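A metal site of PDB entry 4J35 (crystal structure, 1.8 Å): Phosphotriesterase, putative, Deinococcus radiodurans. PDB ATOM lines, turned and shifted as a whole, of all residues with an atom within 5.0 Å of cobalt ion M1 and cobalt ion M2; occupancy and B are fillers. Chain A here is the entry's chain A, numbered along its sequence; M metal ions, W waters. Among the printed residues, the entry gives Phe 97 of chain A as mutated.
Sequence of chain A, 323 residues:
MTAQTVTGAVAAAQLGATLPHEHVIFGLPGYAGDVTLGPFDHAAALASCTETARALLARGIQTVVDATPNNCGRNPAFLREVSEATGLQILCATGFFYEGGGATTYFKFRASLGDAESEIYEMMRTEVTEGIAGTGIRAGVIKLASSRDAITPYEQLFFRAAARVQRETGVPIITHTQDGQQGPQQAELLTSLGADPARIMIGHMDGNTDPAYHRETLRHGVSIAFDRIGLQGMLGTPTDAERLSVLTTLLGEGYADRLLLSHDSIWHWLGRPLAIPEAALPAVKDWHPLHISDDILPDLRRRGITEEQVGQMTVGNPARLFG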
ATOM      1  N   HIS A  21      -7.562  29.133  14.365  1.00  0.00           N
ATOM      2  CA  HIS A  21      -8.855  29.362  13.727  1.00  0.00           C
ATOM      3  C   HIS A  21      -9.524  30.566  14.395  1.00  0.00           C
ATOM      4  O   HIS A  21     -10.138  30.407  15.435  1.00  0.00           O
ATOM      5  CB  HIS A  21      -9.813  28.180  13.869  1.00  0.00           C
ATOM      6  CG  HIS A  21     -11.046  28.304  13.029  1.00  0.00           C
ATOM      7  ND1 HIS A  21     -11.460  27.319  12.141  1.00  0.00           N
ATOM      8  CD2 HIS A  21     -11.993  29.271  12.945  1.00  0.00           C
ATOM      9  CE1 HIS A  21     -12.571  27.698  11.560  1.00  0.00           C
ATOM     10  NE2 HIS A  21     -12.944  28.856  12.077  1.00  0.00           N
ATOM     11  N   HIS A  23     -11.226  34.839  13.174  1.00  0.00           N
ATOM     12  CA  HIS A  23     -11.743  35.679  12.106  1.00  0.00           C
ATOM     13  C   HIS A  23     -11.437  37.161  12.470  1.00  0.00           C
ATOM     14  O   HIS A  23     -12.105  37.720  13.308  1.00  0.00           O
ATOM     15  CB  HIS A  23     -13.264  35.414  11.917  1.00  0.00           C
ATOM     16  CG  HIS A  23     -13.551  33.998  11.450  1.00  0.00           C
ATOM     17  ND1 HIS A  23     -13.283  33.605  10.154  1.00  0.00           N
ATOM     18  CD2 HIS A  23     -14.012  32.891  12.084  1.00  0.00           C
ATOM     19  CE1 HIS A  23     -13.595  32.338  10.006  1.00  0.00           C
ATOM     20  NE2 HIS A  23     -13.993  31.852  11.173  1.00  0.00           N
ATOM     21  N   ALA A  67      -9.424  32.063   9.269  1.00  0.00           N
ATOM     22  CA  ALA A  67     -10.115  30.956   8.554  1.00  0.00           C
ATOM     23  C   ALA A  67     -11.259  31.450   7.682  1.00  0.00           C
ATOM     24  O   ALA A  67     -12.083  30.682   7.213  1.00  0.00           O
ATOM     25  CB  ALA A  67     -10.635  29.983   9.574  1.00  0.00           C
ATOM     26  N   PHE A  97     -17.752  28.598   1.978  1.00  0.00           N
ATOM     27  CA  PHE A  97     -18.432  28.099   3.186  1.00  0.00           C
ATOM     28  C   PHE A  97     -19.468  27.002   2.879  1.00  0.00           C
ATOM     29  O   PHE A  97     -19.878  26.834   1.737  1.00  0.00           O
ATOM     30  CB  PHE A  97     -19.093  29.309   3.863  1.00  0.00           C
ATOM     31  CG  PHE A  97     -19.348  29.152   5.317  1.00  0.00           C
ATOM     32  CD1 PHE A  97     -18.361  28.700   6.196  1.00  0.00           C
ATOM     33  CD2 PHE A  97     -20.567  29.575   5.844  1.00  0.00           C
ATOM     34  CE1 PHE A  97     -18.602  28.617   7.570  1.00  0.00           C
ATOM     35  CE2 PHE A  97     -20.806  29.500   7.234  1.00  0.00           C
ATOM     36  CZ  PHE A  97     -19.819  29.021   8.086  1.00  0.00           C
ATOM     37  N   KCX A 143      -9.506  26.174   3.338  1.00  0.00           N
ATOM     38  CA  KCX A 143     -10.664  26.087   4.197  1.00  0.00           C
ATOM     39  CB  KCX A 143     -11.146  27.461   4.682  1.00  0.00           C
ATOM     40  CG  KCX A 143     -12.447  27.439   5.458  1.00  0.00           C
ATOM     41  CD  KCX A 143     -12.292  26.938   6.896  1.00  0.00           C
ATOM     42  CE  KCX A 143     -13.633  26.908   7.605  1.00  0.00           C
ATOM     43  NZ  KCX A 143     -13.914  28.288   8.266  1.00  0.00           N
ATOM     44  C   KCX A 143     -11.766  25.299   3.516  1.00  0.00           C
ATOM     45  O   KCX A 143     -12.258  25.651   2.424  1.00  0.00           O
ATOM     46  CX  KCX A 143     -14.681  28.577   9.289  1.00  0.00           C
ATOM     47  OQ1 KCX A 143     -14.655  29.822   9.533  1.00  0.00           O
ATOM     48  OQ2 KCX A 143     -15.445  27.830   9.976  1.00  0.00           O
ATOM     49  N   HIS A 176     -14.367  23.297   8.778  1.00  0.00           N
ATOM     50  CA  HIS A 176     -15.535  23.593   9.573  1.00  0.00           C
ATOM     51  C   HIS A 176     -16.416  22.344   9.614  1.00  0.00           C
ATOM     52  O   HIS A 176     -16.680  21.759   8.566  1.00  0.00           O
ATOM     53  CB  HIS A 176     -16.300  24.755   8.907  1.00  0.00           C
ATOM     54  CG  HIS A 176     -17.709  24.974   9.403  1.00  0.00           C
ATOM     55  ND1 HIS A 176     -18.092  26.050  10.151  1.00  0.00           N
ATOM     56  CD2 HIS A 176     -18.852  24.278   9.145  1.00  0.00           C
ATOM     57  CE1 HIS A 176     -19.395  25.991  10.396  1.00  0.00           C
ATOM     58  NE2 HIS A 176     -19.876  24.927   9.808  1.00  0.00           N
ATOM     59  N   HIS A 204     -13.859  22.559  14.626  1.00  0.00           N
ATOM     60  CA  HIS A 204     -15.057  22.595  15.446  1.00  0.00           C
ATOM     61  C   HIS A 204     -15.385  21.255  16.111  1.00  0.00           C
ATOM     62  O   HIS A 204     -16.564  20.931  16.339  1.00  0.00           O
ATOM     63  CB  HIS A 204     -16.258  23.147  14.638  1.00  0.00           C
ATOM     64  CG  HIS A 204     -16.007  24.444  13.926  1.00  0.00           C
ATOM     65  ND1 HIS A 204     -15.073  25.369  14.349  1.00  0.00           N
ATOM     66  CD2 HIS A 204     -16.587  24.981  12.825  1.00  0.00           C
ATOM     67  CE1 HIS A 204     -15.096  26.424  13.538  1.00  0.00           C
ATOM     68  NE2 HIS A 204     -16.001  26.199  12.597  1.00  0.00           N
ATOM     69  N   ASP A 264     -12.478  30.755  17.321  1.00  0.00           N
ATOM     70  CA  ASP A 264     -13.396  31.081  16.223  1.00  0.00           C
ATOM     71  C   ASP A 264     -14.037  32.460  16.470  1.00  0.00           C
ATOM     72  O   ASP A 264     -15.181  32.700  16.114  1.00  0.00           O
ATOM     73  CB  ASP A 264     -14.473  30.021  16.114  1.00  0.00           C
ATOM     74  CG  ASP A 264     -15.190  30.042  14.766  1.00  0.00           C
ATOM     75  OD1 ASP A 264     -14.719  30.661  13.790  1.00  0.00           O
ATOM     76  OD2 ASP A 264     -16.276  29.448  14.715  1.00  0.00           O
HETATM   77 CO    CO M   1     -16.703  27.366  11.131  1.00  0.00          CO
HETATM   78 CO    CO M   2     -14.665  30.072  11.659  1.00  0.00          CO
HETATM   79  O   HOH W   1     -18.977  27.586  13.099  1.00  0.00           O
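Within 4 Å of cobalt ion M1: KCX 143, His 176 and His 204.
Of the 8 residues printed, 4 come within 4 Å of cobalt ion M2. The nearest printed residue that does not touch cobalt ion M2 is His 204 (4.1 Å).
The backbone carbonyl oxygen (O) of Ala 67 is in hydrogen-bond range of NZ of KCX 143, at 3.2 Å.
Cobalt ion M1 is bound by OQ2 of KCX 143, a ring nitrogen (NE2) of His 204 and a ring nitrogen (ND1) of His 176. Cobalt ion M1 has three donor atoms within binding distance.
Cobalt ion M2 is bound by a ring nitrogen (NE2) of His 23 (2.0 Å), OQ1 of KCX 143 (2.1 Å), a ring nitrogen (NE2) of His 21 (2.1 Å) and the side-chain carboxylate of Asp 264 (2.2 Å).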
